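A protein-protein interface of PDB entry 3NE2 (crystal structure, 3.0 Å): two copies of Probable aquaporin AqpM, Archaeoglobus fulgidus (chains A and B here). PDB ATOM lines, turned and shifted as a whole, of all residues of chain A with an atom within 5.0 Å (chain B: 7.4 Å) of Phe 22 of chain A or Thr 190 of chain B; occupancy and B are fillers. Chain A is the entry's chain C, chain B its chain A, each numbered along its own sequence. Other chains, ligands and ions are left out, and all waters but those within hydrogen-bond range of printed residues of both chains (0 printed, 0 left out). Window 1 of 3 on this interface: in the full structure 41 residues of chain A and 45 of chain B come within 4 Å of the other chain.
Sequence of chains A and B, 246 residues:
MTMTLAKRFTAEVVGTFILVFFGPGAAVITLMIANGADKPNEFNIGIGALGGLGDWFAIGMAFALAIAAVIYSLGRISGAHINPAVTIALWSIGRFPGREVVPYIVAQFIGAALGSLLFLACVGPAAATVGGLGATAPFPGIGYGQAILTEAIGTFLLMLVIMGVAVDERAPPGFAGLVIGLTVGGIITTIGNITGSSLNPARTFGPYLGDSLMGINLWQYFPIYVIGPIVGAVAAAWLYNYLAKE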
ATOM      1  N   PHE A  17      16.207  34.333   8.242  1.00  0.00           N
ATOM      2  CA  PHE A  17      14.826  34.046   8.574  1.00  0.00           C
ATOM      3  C   PHE A  17      14.650  32.585   8.984  1.00  0.00           C
ATOM      4  O   PHE A  17      14.074  32.296  10.011  1.00  0.00           O
ATOM      5  CB  PHE A  17      13.925  34.387   7.377  1.00  0.00           C
ATOM      6  CG  PHE A  17      12.595  33.705   7.414  1.00  0.00           C
ATOM      7  CD1 PHE A  17      12.415  32.500   6.758  1.00  0.00           C
ATOM      8  CD2 PHE A  17      11.533  34.262   8.122  1.00  0.00           C
ATOM      9  CE1 PHE A  17      11.200  31.858   6.806  1.00  0.00           C
ATOM     10  CE2 PHE A  17      10.318  33.632   8.176  1.00  0.00           C
ATOM     11  CZ  PHE A  17      10.145  32.425   7.526  1.00  0.00           C
ATOM     12  N   ILE A  18      15.153  31.676   8.161  1.00  0.00           N
ATOM     13  CA  ILE A  18      15.066  30.242   8.442  1.00  0.00           C
ATOM     14  C   ILE A  18      15.906  29.863   9.663  1.00  0.00           C
ATOM     15  O   ILE A  18      15.476  29.033  10.485  1.00  0.00           O
ATOM     16  CB  ILE A  18      15.453  29.394   7.212  1.00  0.00           C
ATOM     17  CG1 ILE A  18      14.246  29.306   6.283  1.00  0.00           C
ATOM     18  CG2 ILE A  18      15.916  28.006   7.606  1.00  0.00           C
ATOM     19  CD1 ILE A  18      14.607  29.298   4.850  1.00  0.00           C
ATOM     20  N   LEU A  19      17.078  30.487   9.804  1.00  0.00           N
ATOM     21  CA  LEU A  19      17.899  30.301  11.005  1.00  0.00           C
ATOM     22  C   LEU A  19      17.109  30.628  12.264  1.00  0.00           C
ATOM     23  O   LEU A  19      17.074  29.808  13.170  1.00  0.00           O
ATOM     24  CB  LEU A  19      19.159  31.173  11.006  1.00  0.00           C
ATOM     25  CG  LEU A  19      19.927  31.242  12.353  1.00  0.00           C
ATOM     26  CD1 LEU A  19      20.394  29.842  12.761  1.00  0.00           C
ATOM     27  CD2 LEU A  19      21.115  32.215  12.314  1.00  0.00           C
ATOM     28  N   VAL A  20      16.467  31.803  12.327  1.00  0.00           N
ATOM     29  CA  VAL A  20      15.697  32.173  13.547  1.00  0.00           C
ATOM     30  C   VAL A  20      14.267  31.566  13.662  1.00  0.00           C
ATOM     31  O   VAL A  20      13.683  31.543  14.757  1.00  0.00           O
ATOM     32  CB  VAL A  20      15.590  33.688  13.748  1.00  0.00           C
ATOM     33  CG1 VAL A  20      16.997  34.300  13.839  1.00  0.00           C
ATOM     34  CG2 VAL A  20      14.769  34.307  12.630  1.00  0.00           C
ATOM     35  N   PHE A  21      13.700  31.062  12.563  1.00  0.00           N
ATOM     36  CA  PHE A  21      12.364  30.492  12.638  1.00  0.00           C
ATOM     37  C   PHE A  21      12.511  29.170  13.326  1.00  0.00           C
ATOM     38  O   PHE A  21      11.906  28.939  14.357  1.00  0.00           O
ATOM     39  CB  PHE A  21      11.726  30.326  11.259  1.00  0.00           C
ATOM     40  CG  PHE A  21      10.328  29.835  11.318  1.00  0.00           C
ATOM     41  CD1 PHE A  21      10.062  28.489  11.501  1.00  0.00           C
ATOM     42  CD2 PHE A  21       9.262  30.721  11.231  1.00  0.00           C
ATOM     43  CE1 PHE A  21       8.747  28.017  11.586  1.00  0.00           C
ATOM     44  CE2 PHE A  21       7.931  30.259  11.316  1.00  0.00           C
ATOM     45  CZ  PHE A  21       7.676  28.900  11.503  1.00  0.00           C
ATOM     46  N   PHE A  22      13.383  28.338  12.772  1.00  0.00           N
ATOM     47  CA  PHE A  22      13.480  26.940  13.166  1.00  0.00           C
ATOM     48  C   PHE A  22      14.430  26.727  14.340  1.00  0.00           C
ATOM     49  O   PHE A  22      14.157  25.916  15.225  1.00  0.00           O
ATOM     50  CB  PHE A  22      13.960  26.100  11.984  1.00  0.00           C
ATOM     51  CG  PHE A  22      12.919  25.917  10.896  1.00  0.00           C
ATOM     52  CD1 PHE A  22      12.145  24.771  10.832  1.00  0.00           C
ATOM     53  CD2 PHE A  22      12.733  26.886   9.936  1.00  0.00           C
ATOM     54  CE1 PHE A  22      11.209  24.604   9.835  1.00  0.00           C
ATOM     55  CE2 PHE A  22      11.784  26.715   8.956  1.00  0.00           C
ATOM     56  CZ  PHE A  22      11.028  25.565   8.910  1.00  0.00           C
ATOM     57  N   GLY A  23      15.554  27.433  14.345  1.00  0.00           N
ATOM     58  CA  GLY A  23      16.536  27.270  15.411  1.00  0.00           C
ATOM     59  C   GLY A  23      15.926  27.553  16.766  1.00  0.00           C
ATOM     60  O   GLY A  23      15.687  26.622  17.529  1.00  0.00           O
ATOM     61  N   PRO A  24      15.662  28.838  17.077  1.00  0.00           N
ATOM     62  CA  PRO A  24      15.028  29.209  18.365  1.00  0.00           C
ATOM     63  C   PRO A  24      13.566  28.723  18.508  1.00  0.00           C
ATOM     64  O   PRO A  24      12.999  28.733  19.620  1.00  0.00           O
ATOM     65  CB  PRO A  24      15.101  30.749  18.376  1.00  0.00           C
ATOM     66  CG  PRO A  24      16.204  31.088  17.426  1.00  0.00           C
ATOM     67  CD  PRO A  24      16.145  30.024  16.354  1.00  0.00           C
ATOM     68  N   GLY A  25      12.972  28.314  17.378  1.00  0.00           N
ATOM     69  CA  GLY A  25      11.621  27.749  17.357  1.00  0.00           C
ATOM     70  C   GLY A  25      11.521  26.416  18.083  1.00  0.00           C
ATOM     71  O   GLY A  25      10.505  26.127  18.716  1.00  0.00           O
ATOM     72  N   ALA A  26      12.572  25.601  17.982  1.00  0.00           N
ATOM     73  CA  ALA A  26      12.680  24.355  18.760  1.00  0.00           C
ATOM     74  C   ALA A  26      12.768  24.638  20.264  1.00  0.00           C
ATOM     75  O   ALA A  26      12.116  23.962  21.071  1.00  0.00           O
ATOM     76  CB  ALA A  26      13.890  23.550  18.322  1.00  0.00           C
ATOM     77  N   ILE A  29       9.290  25.392  21.526  1.00  0.00           N
ATOM     78  CA  ILE A  29       8.457  24.191  21.570  1.00  0.00           C
ATOM     79  C   ILE A  29       8.894  23.251  22.682  1.00  0.00           C
ATOM     80  O   ILE A  29       8.033  22.629  23.317  1.00  0.00           O
ATOM     81  CB  ILE A  29       8.411  23.470  20.211  1.00  0.00           C
ATOM     82  CG1 ILE A  29       7.582  24.312  19.227  1.00  0.00           C
ATOM     83  CG2 ILE A  29       7.819  22.072  20.344  1.00  0.00           C
ATOM     84  CD1 ILE A  29       6.074  24.219  19.440  1.00  0.00           C
ATOM     85  N   ALA A  62      18.008  20.929  15.497  1.00  0.00           N
ATOM     86  CA  ALA A  62      17.059  21.838  14.842  1.00  0.00           C
ATOM     87  C   ALA A  62      17.796  23.026  14.220  1.00  0.00           C
ATOM     88  O   ALA A  62      17.554  23.372  13.074  1.00  0.00           O
ATOM     89  CB  ALA A  62      16.031  22.341  15.833  1.00  0.00           C
ATOM     90  N   ALA A  66      19.005  23.051   9.953  1.00  0.00           N
ATOM     91  CA  ALA A  66      18.488  24.262   9.303  1.00  0.00           C
ATOM     92  C   ALA A  66      19.634  25.114   8.695  1.00  0.00           C
ATOM     93  O   ALA A  66      19.589  25.552   7.529  1.00  0.00           O
ATOM     94  CB  ALA A  66      17.725  25.084  10.285  1.00  0.00           C
ATOM     95  N   PHE A 119       7.236  32.912  13.364  1.00  0.00           N
ATOM     96  CA  PHE A 119       7.066  31.812  14.328  1.00  0.00           C
ATOM     97  C   PHE A 119       6.003  32.176  15.375  1.00  0.00           C
ATOM     98  O   PHE A 119       5.094  31.401  15.623  1.00  0.00           O
ATOM     99  CB  PHE A 119       8.380  31.447  15.028  1.00  0.00           C
ATOM    100  CG  PHE A 119       8.324  30.119  15.750  1.00  0.00           C
ATOM    101  CD1 PHE A 119       8.682  28.934  15.101  1.00  0.00           C
ATOM    102  CD2 PHE A 119       7.889  30.044  17.071  1.00  0.00           C
ATOM    103  CE1 PHE A 119       8.628  27.687  15.759  1.00  0.00           C
ATOM    104  CE2 PHE A 119       7.831  28.802  17.734  1.00  0.00           C
ATOM    105  CZ  PHE A 119       8.208  27.622  17.068  1.00  0.00           C
ATOM    106  N   LEU B  53      11.717  17.054  23.902  1.00  0.00           N
ATOM    107  CA  LEU B  53      11.874  17.363  22.482  1.00  0.00           C
ATOM    108  C   LEU B  53      12.744  16.312  21.788  1.00  0.00           C
ATOM    109  O   LEU B  53      12.682  16.136  20.555  1.00  0.00           O
ATOM    110  CB  LEU B  53      12.496  18.749  22.302  1.00  0.00           C
ATOM    111  CG  LEU B  53      12.352  19.347  20.906  1.00  0.00           C
ATOM    112  CD1 LEU B  53      10.940  19.909  20.714  1.00  0.00           C
ATOM    113  CD2 LEU B  53      13.416  20.409  20.673  1.00  0.00           C
ATOM    114  N   TRP B  56      10.751  14.236  19.673  1.00  0.00           N
ATOM    115  CA  TRP B  56      10.516  14.800  18.365  1.00  0.00           C
ATOM    116  C   TRP B  56      11.717  14.637  17.452  1.00  0.00           C
ATOM    117  O   TRP B  56      11.528  14.375  16.274  1.00  0.00           O
ATOM    118  CB  TRP B  56      10.113  16.271  18.460  1.00  0.00           C
ATOM    119  CG  TRP B  56       8.653  16.495  18.587  1.00  0.00           C
ATOM    120  CD1 TRP B  56       8.031  17.190  19.572  1.00  0.00           C
ATOM    121  CD2 TRP B  56       7.619  16.044  17.697  1.00  0.00           C
ATOM    122  NE1 TRP B  56       6.668  17.204  19.367  1.00  0.00           N
ATOM    123  CE2 TRP B  56       6.390  16.506  18.220  1.00  0.00           C
ATOM    124  CE3 TRP B  56       7.608  15.296  16.521  1.00  0.00           C
ATOM    125  CZ2 TRP B  56       5.149  16.239  17.599  1.00  0.00           C
ATOM    126  CZ3 TRP B  56       6.388  15.041  15.893  1.00  0.00           C
ATOM    127  CH2 TRP B  56       5.175  15.515  16.430  1.00  0.00           C
ATOM    128  N   PHE B  57      12.938  14.804  17.967  1.00  0.00           N
ATOM    129  CA  PHE B  57      14.154  14.632  17.120  1.00  0.00           C
ATOM    130  C   PHE B  57      14.330  13.164  16.698  1.00  0.00           C
ATOM    131  O   PHE B  57      14.674  12.867  15.532  1.00  0.00           O
ATOM    132  CB  PHE B  57      15.421  15.147  17.821  1.00  0.00           C
ATOM    133  CG  PHE B  57      16.689  14.964  17.009  1.00  0.00           C
ATOM    134  CD1 PHE B  57      16.912  15.703  15.859  1.00  0.00           C
ATOM    135  CD2 PHE B  57      17.661  14.045  17.408  1.00  0.00           C
ATOM    136  CE1 PHE B  57      18.084  15.530  15.121  1.00  0.00           C
ATOM    137  CE2 PHE B  57      18.826  13.867  16.677  1.00  0.00           C
ATOM    138  CZ  PHE B  57      19.042  14.608  15.532  1.00  0.00           C
ATOM    139  N   THR B 150       2.313  27.292   8.888  1.00  0.00           N
ATOM    140  CA  THR B 150       3.474  26.591   9.410  1.00  0.00           C
ATOM    141  C   THR B 150       3.850  25.428   8.480  1.00  0.00           C
ATOM    142  O   THR B 150       5.020  25.073   8.384  1.00  0.00           O
ATOM    143  CB  THR B 150       3.256  26.037  10.809  1.00  0.00           C
ATOM    144  OG1 THR B 150       2.568  24.789  10.710  1.00  0.00           O
ATOM    145  CG2 THR B 150       2.464  27.015  11.675  1.00  0.00           C
ATOM    146  N   ALA B 152       3.382  25.566   5.227  1.00  0.00           N
ATOM    147  CA  ALA B 152       3.973  26.201   4.072  1.00  0.00           C
ATOM    148  C   ALA B 152       5.417  26.572   4.398  1.00  0.00           C
ATOM    149  O   ALA B 152       6.338  26.230   3.649  1.00  0.00           O
ATOM    150  CB  ALA B 152       3.150  27.436   3.658  1.00  0.00           C
ATOM    151  N   ILE B 153       5.617  27.251   5.526  1.00  0.00           N
ATOM    152  CA  ILE B 153       6.960  27.675   5.931  1.00  0.00           C
ATOM    153  C   ILE B 153       7.850  26.483   6.070  1.00  0.00           C
ATOM    154  O   ILE B 153       9.020  26.573   5.848  1.00  0.00           O
ATOM    155  CB  ILE B 153       6.946  28.453   7.266  1.00  0.00           C
ATOM    156  CG1 ILE B 153       6.350  29.849   7.050  1.00  0.00           C
ATOM    157  CG2 ILE B 153       8.368  28.537   7.866  1.00  0.00           C
ATOM    158  CD1 ILE B 153       6.142  30.616   8.320  1.00  0.00           C
ATOM    159  N   GLY B 154       7.260  25.363   6.443  1.00  0.00           N
ATOM    160  CA  GLY B 154       7.971  24.094   6.601  1.00  0.00           C
ATOM    161  C   GLY B 154       8.437  23.551   5.284  1.00  0.00           C
ATOM    162  O   GLY B 154       9.629  23.314   5.125  1.00  0.00           O
ATOM    163  N   THR B 155       7.500  23.392   4.339  1.00  0.00           N
ATOM    164  CA  THR B 155       7.775  22.762   3.033  1.00  0.00           C
ATOM    165  C   THR B 155       8.538  23.711   2.087  1.00  0.00           C
ATOM    166  O   THR B 155       9.093  23.310   1.036  1.00  0.00           O
ATOM    167  CB  THR B 155       6.468  22.263   2.376  1.00  0.00           C
ATOM    168  OG1 THR B 155       5.544  21.836   3.389  1.00  0.00           O
ATOM    169  CG2 THR B 155       6.764  21.086   1.452  1.00  0.00           C
ATOM    170  N   PHE B 156       8.553  24.984   2.470  1.00  0.00           N
ATOM    171  CA  PHE B 156       9.324  25.986   1.758  1.00  0.00           C
ATOM    172  C   PHE B 156      10.788  25.752   1.932  1.00  0.00           C
ATOM    173  O   PHE B 156      11.520  25.816   0.960  1.00  0.00           O
ATOM    174  CB  PHE B 156       8.969  27.383   2.262  1.00  0.00           C
ATOM    175  CG  PHE B 156       9.939  28.444   1.827  1.00  0.00           C
ATOM    176  CD1 PHE B 156       9.813  29.059   0.565  1.00  0.00           C
ATOM    177  CD2 PHE B 156      10.961  28.840   2.680  1.00  0.00           C
ATOM    178  CE1 PHE B 156      10.700  30.043   0.166  1.00  0.00           C
ATOM    179  CE2 PHE B 156      11.857  29.816   2.286  1.00  0.00           C
ATOM    180  CZ  PHE B 156      11.736  30.422   1.026  1.00  0.00           C
ATOM    181  N   LEU B 157      11.204  25.513   3.178  1.00  0.00           N
ATOM    182  CA  LEU B 157      12.596  25.208   3.485  1.00  0.00           C
ATOM    183  C   LEU B 157      13.000  23.878   2.860  1.00  0.00           C
ATOM    184  O   LEU B 157      14.072  23.779   2.310  1.00  0.00           O
ATOM    185  CB  LEU B 157      12.863  25.180   4.990  1.00  0.00           C
ATOM    186  CG  LEU B 157      14.326  24.868   5.327  1.00  0.00           C
ATOM    187  CD1 LEU B 157      15.208  25.979   4.860  1.00  0.00           C
ATOM    188  CD2 LEU B 157      14.522  24.667   6.768  1.00  0.00           C
ATOM    189  N   LEU B 158      12.157  22.856   2.946  1.00  0.00           N
ATOM    190  CA  LEU B 158      12.446  21.604   2.260  1.00  0.00           C
ATOM    191  C   LEU B 158      12.760  21.845   0.776  1.00  0.00           C
ATOM    192  O   LEU B 158      13.864  21.572   0.313  1.00  0.00           O
ATOM    193  CB  LEU B 158      11.284  20.610   2.407  1.00  0.00           C
ATOM    194  CG  LEU B 158      11.369  19.298   1.587  1.00  0.00           C
ATOM    195  CD1 LEU B 158      12.794  18.667   1.586  1.00  0.00           C
ATOM    196  CD2 LEU B 158      10.273  18.277   2.081  1.00  0.00           C
ATOM    197  N   THR B 183      17.524  17.557   6.598  1.00  0.00           N
ATOM    198  CA  THR B 183      16.798  18.809   6.599  1.00  0.00           C
ATOM    199  C   THR B 183      15.395  18.591   7.079  1.00  0.00           C
ATOM    200  O   THR B 183      14.931  19.344   7.936  1.00  0.00           O
ATOM    201  CB  THR B 183      16.721  19.425   5.207  1.00  0.00           C
ATOM    202  OG1 THR B 183      18.040  19.688   4.702  1.00  0.00           O
ATOM    203  CG2 THR B 183      15.845  20.735   5.231  1.00  0.00           C
ATOM    204  N   VAL B 184      14.717  17.586   6.518  1.00  0.00           N
ATOM    205  CA  VAL B 184      13.357  17.210   6.970  1.00  0.00           C
ATOM    206  C   VAL B 184      13.357  16.957   8.477  1.00  0.00           C
ATOM    207  O   VAL B 184      12.555  17.508   9.226  1.00  0.00           O
ATOM    208  CB  VAL B 184      12.829  15.918   6.226  1.00  0.00           C
ATOM    209  CG1 VAL B 184      11.637  15.310   6.945  1.00  0.00           C
ATOM    210  CG2 VAL B 184      12.506  16.217   4.729  1.00  0.00           C
ATOM    211  N   GLY B 185      14.305  16.115   8.885  1.00  0.00           N
ATOM    212  CA  GLY B 185      14.507  15.742  10.285  1.00  0.00           C
ATOM    213  C   GLY B 185      14.490  16.965  11.168  1.00  0.00           C
ATOM    214  O   GLY B 185      13.792  17.005  12.219  1.00  0.00           O
ATOM    215  N   GLY B 186      15.240  17.970  10.731  1.00  0.00           N
ATOM    216  CA  GLY B 186      15.285  19.261  11.435  1.00  0.00           C
ATOM    217  C   GLY B 186      13.932  19.976  11.534  1.00  0.00           C
ATOM    218  O   GLY B 186      13.559  20.471  12.599  1.00  0.00           O
ATOM    219  N   ILE B 187      13.215  20.032  10.410  1.00  0.00           N
ATOM    220  CA  ILE B 187      11.922  20.716  10.344  1.00  0.00           C
ATOM    221  C   ILE B 187      10.940  20.051  11.340  1.00  0.00           C
ATOM    222  O   ILE B 187      10.290  20.729  12.156  1.00  0.00           O
ATOM    223  CB  ILE B 187      11.357  20.710   8.871  1.00  0.00           C
ATOM    224  CG1 ILE B 187      12.311  21.434   7.933  1.00  0.00           C
ATOM    225  CG2 ILE B 187       9.999  21.366   8.785  1.00  0.00           C
ATOM    226  CD1 ILE B 187      12.190  20.998   6.497  1.00  0.00           C
ATOM    227  N   ILE B 188      10.860  18.719  11.285  1.00  0.00           N
ATOM    228  CA  ILE B 188       9.957  17.988  12.153  1.00  0.00           C
ATOM    229  C   ILE B 188      10.254  18.353  13.595  1.00  0.00           C
ATOM    230  O   ILE B 188       9.355  18.660  14.321  1.00  0.00           O
ATOM    231  CB  ILE B 188      10.042  16.462  11.941  1.00  0.00           C
ATOM    232  CG1 ILE B 188       9.517  16.096  10.543  1.00  0.00           C
ATOM    233  CG2 ILE B 188       9.247  15.732  13.027  1.00  0.00           C
ATOM    234  CD1 ILE B 188       9.390  14.606  10.267  1.00  0.00           C
ATOM    235  N   THR B 189      11.522  18.367  13.989  1.00  0.00           N
ATOM    236  CA  THR B 189      11.895  18.755  15.349  1.00  0.00           C
ATOM    237  C   THR B 189      11.221  20.086  15.824  1.00  0.00           C
ATOM    238  O   THR B 189      10.664  20.172  16.927  1.00  0.00           O
ATOM    239  CB  THR B 189      13.437  18.786  15.501  1.00  0.00           C
ATOM    240  OG1 THR B 189      13.927  17.448  15.343  1.00  0.00           O
ATOM    241  CG2 THR B 189      13.860  19.379  16.881  1.00  0.00           C
ATOM    242  N   THR B 190      11.239  21.112  14.994  1.00  0.00           N
ATOM    243  CA  THR B 190      10.609  22.374  15.379  1.00  0.00           C
ATOM    244  C   THR B 190       9.081  22.362  15.148  1.00  0.00           C
ATOM    245  O   THR B 190       8.299  22.697  16.054  1.00  0.00           O
ATOM    246  CB  THR B 190      11.170  23.546  14.593  1.00  0.00           C
ATOM    247  OG1 THR B 190      12.595  23.544  14.654  1.00  0.00           O
ATOM    248  CG2 THR B 190      10.644  24.833  15.167  1.00  0.00           C
ATOM    249  N   ILE B 191       8.666  21.980  13.932  1.00  0.00           N
ATOM    250  CA  ILE B 191       7.271  22.101  13.487  1.00  0.00           C
ATOM    251  C   ILE B 191       6.354  20.972  13.979  1.00  0.00           C
ATOM    252  O   ILE B 191       5.118  21.103  13.955  1.00  0.00           O
ATOM    253  CB  ILE B 191       7.231  22.160  11.962  1.00  0.00           C
ATOM    254  CG1 ILE B 191       7.819  23.481  11.497  1.00  0.00           C
ATOM    255  CG2 ILE B 191       5.829  22.076  11.444  1.00  0.00           C
ATOM    256  CD1 ILE B 191       7.013  24.709  11.958  1.00  0.00           C
ATOM    257  N   GLY B 192       6.969  19.882  14.445  1.00  0.00           N
ATOM    258  CA  GLY B 192       6.269  18.657  14.850  1.00  0.00           C
ATOM    259  C   GLY B 192       5.120  18.886  15.792  1.00  0.00           C
ATOM    260  O   GLY B 192       4.012  18.429  15.544  1.00  0.00           O
ATOM    261  N   ASN B 193       5.361  19.596  16.881  1.00  0.00           N
ATOM    262  CA  ASN B 193       4.305  19.791  17.853  1.00  0.00           C
ATOM    263  C   ASN B 193       3.378  20.944  17.498  1.00  0.00           C
ATOM    264  O   ASN B 193       2.607  21.390  18.350  1.00  0.00           O
ATOM    265  CB  ASN B 193       4.893  20.001  19.240  1.00  0.00           C
ATOM    266  CG  ASN B 193       3.977  19.517  20.325  1.00  0.00           C
ATOM    267  OD1 ASN B 193       4.126  18.395  20.796  1.00  0.00           O
ATOM    268  ND2 ASN B 193       3.000  20.350  20.718  1.00  0.00           N
ATOM    269  N   ILE B 194       3.438  21.430  16.266  1.00  0.00           N
ATOM    270  CA  ILE B 194       2.516  22.469  15.827  1.00  0.00           C
ATOM    271  C   ILE B 194       1.502  21.908  14.836  1.00  0.00           C
ATOM    272  O   ILE B 194       0.319  22.243  14.908  1.00  0.00           O
ATOM    273  CB  ILE B 194       3.248  23.688  15.212  1.00  0.00           C
ATOM    274  CG1 ILE B 194       4.254  24.268  16.217  1.00  0.00           C
ATOM    275  CG2 ILE B 194       2.235  24.774  14.809  1.00  0.00           C
ATOM    276  CD1 ILE B 194       5.314  25.177  15.578  1.00  0.00           C
ATOM    277  N   THR B 195       1.956  21.089  13.891  1.00  0.00           N
ATOM    278  CA  THR B 195       1.037  20.482  12.927  1.00  0.00           C
ATOM    279  C   THR B 195       1.319  19.046  12.609  1.00  0.00           C
ATOM    280  O   THR B 195       0.663  18.463  11.763  1.00  0.00           O
ATOM    281  CB  THR B 195       1.056  21.220  11.586  1.00  0.00           C
ATOM    282  OG1 THR B 195       2.264  20.892  10.868  1.00  0.00           O
ATOM    283  CG2 THR B 195       0.889  22.733  11.820  1.00  0.00           C
ATOM    284  N   SER B 197       4.129  18.297  11.341  1.00  0.00           N
ATOM    285  CA  SER B 197       5.149  18.467  10.286  1.00  0.00           C
ATOM    286  C   SER B 197       5.032  17.447   9.134  1.00  0.00           C
ATOM    287  O   SER B 197       5.858  16.570   8.974  1.00  0.00           O
ATOM    288  CB  SER B 197       6.533  18.442  10.930  1.00  0.00           C
ATOM    289  OG  SER B 197       7.472  19.084  10.105  1.00  0.00           O
ATOM    290  N   LEU B 199       4.429  18.192   5.571  1.00  0.00           N
ATOM    291  CA  LEU B 199       5.174  18.704   4.423  1.00  0.00           C
ATOM    292  C   LEU B 199       4.788  17.967   3.141  1.00  0.00           C
ATOM    293  O   LEU B 199       5.429  18.178   2.091  1.00  0.00           O
ATOM    294  CB  LEU B 199       6.710  18.633   4.642  1.00  0.00           C
ATOM    295  CG  LEU B 199       7.398  19.417   5.774  1.00  0.00           C
ATOM    296  CD1 LEU B 199       7.325  18.663   7.093  1.00  0.00           C
ATOM    297  CD2 LEU B 199       8.826  19.642   5.461  1.00  0.00           C
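The side-chain hydroxyl (OG1) of Thr 190 of chain B sits at hydrogen-bond distance from the backbone carbonyl oxygen (O) of Phe 22 of chain A (2.9 Å).
OG1 of Thr 189 of chain B lies within hydrogen-bond range of O of Gly 185 of chain B, 3.2 Å away.
The indole nitrogen (NE1) of Trp 56 of chain B sits at hydrogen-bond distance from the side-chain amide oxygen (OD1) of Asn 193 of chain B, at 3.1 Å.
CD1 of Leu 157 of chain B touches CD1 of Ile 18 of chain A, at 3.4 Å.
CD1 of Ile 191 of chain B touches CE1 of Phe 21 of chain A, 3.8 Å away.
Phe 22 of chain A touches Ile 153 of chain B.
Ile 187 of chain B touches Phe 22 of chain A (CG2 to CE1, 3.6 Å).
Ala 26 of chain A touches Thr 190 of chain B (N to CG2, 3.5 Å).
CG2 of Ile 29 of chain A touches CD1 of Leu 53 of chain B, 3.8 Å away.
Thr 190 of chain B touches Ile 29 of chain A (O to CG1, 3.6 Å).
CB of Asn 193 of chain B touches CG2 of Ile 29 of chain A, 3.8 Å away.
Ile 29 of chain A touches Ile 194 of chain B.
CB of Ala 62 of chain A touches OG1 of Thr 190 of chain B, 3.8 Å away.
Val 20 of chain A touches none of the printed residues of chain B.
Gly 23 of chain A touches none of the printed residues of chain B.
Printed residues of chain B within 4 Å of Phe 119 of chain A: Thr 190 (3.5 Å).
Of the printed residues of chain A, Leu 53 of chain B touches Ala 26 (3.8 Å) and Ile 29 (3.8 Å).
Printed residues of chain A within 4 Å of Thr 190 of chain B: Phe 22 (2.9 Å), Gly 25 (3.4 Å), Ala 26 (3.5 Å), Ile 29 (3.6 Å), Ala 62 (3.8 Å) and Phe 119 (3.5 Å).
The nearest residue of chain B that does not touch Phe 22 of chain A is Leu 157 of chain B (4.1 Å).
The nearest printed residue of chain A that does not touch Ile 187 of chain B is Ala 62 of chain A (6.1 Å).
Hydrophobic or aromatic side chains of chain B that line the printed part of chain A: Leu 53, Ile 153, Phe 156, Leu 157, Ile 187, Ile 191 and Ile 194.
Of the 14 printed residues of chain A, 8 touch a printed residue of chain B.
Printed residues of chain A that touch a printed residue of chain B: Ile 18, Phe 21, Phe 22, Gly 25, Ala 26, Ile 29, Ala 62 and Phe 119.
Hydrophobic or aromatic side chains of chain A that line the printed part of chain B: Ile 18, Phe 21, Phe 22, Ala 26, Ile 29, Ala 62 and Phe 119.
Among the printed residues, 18 pairs touch across the chains.
No position is printed for both chains.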
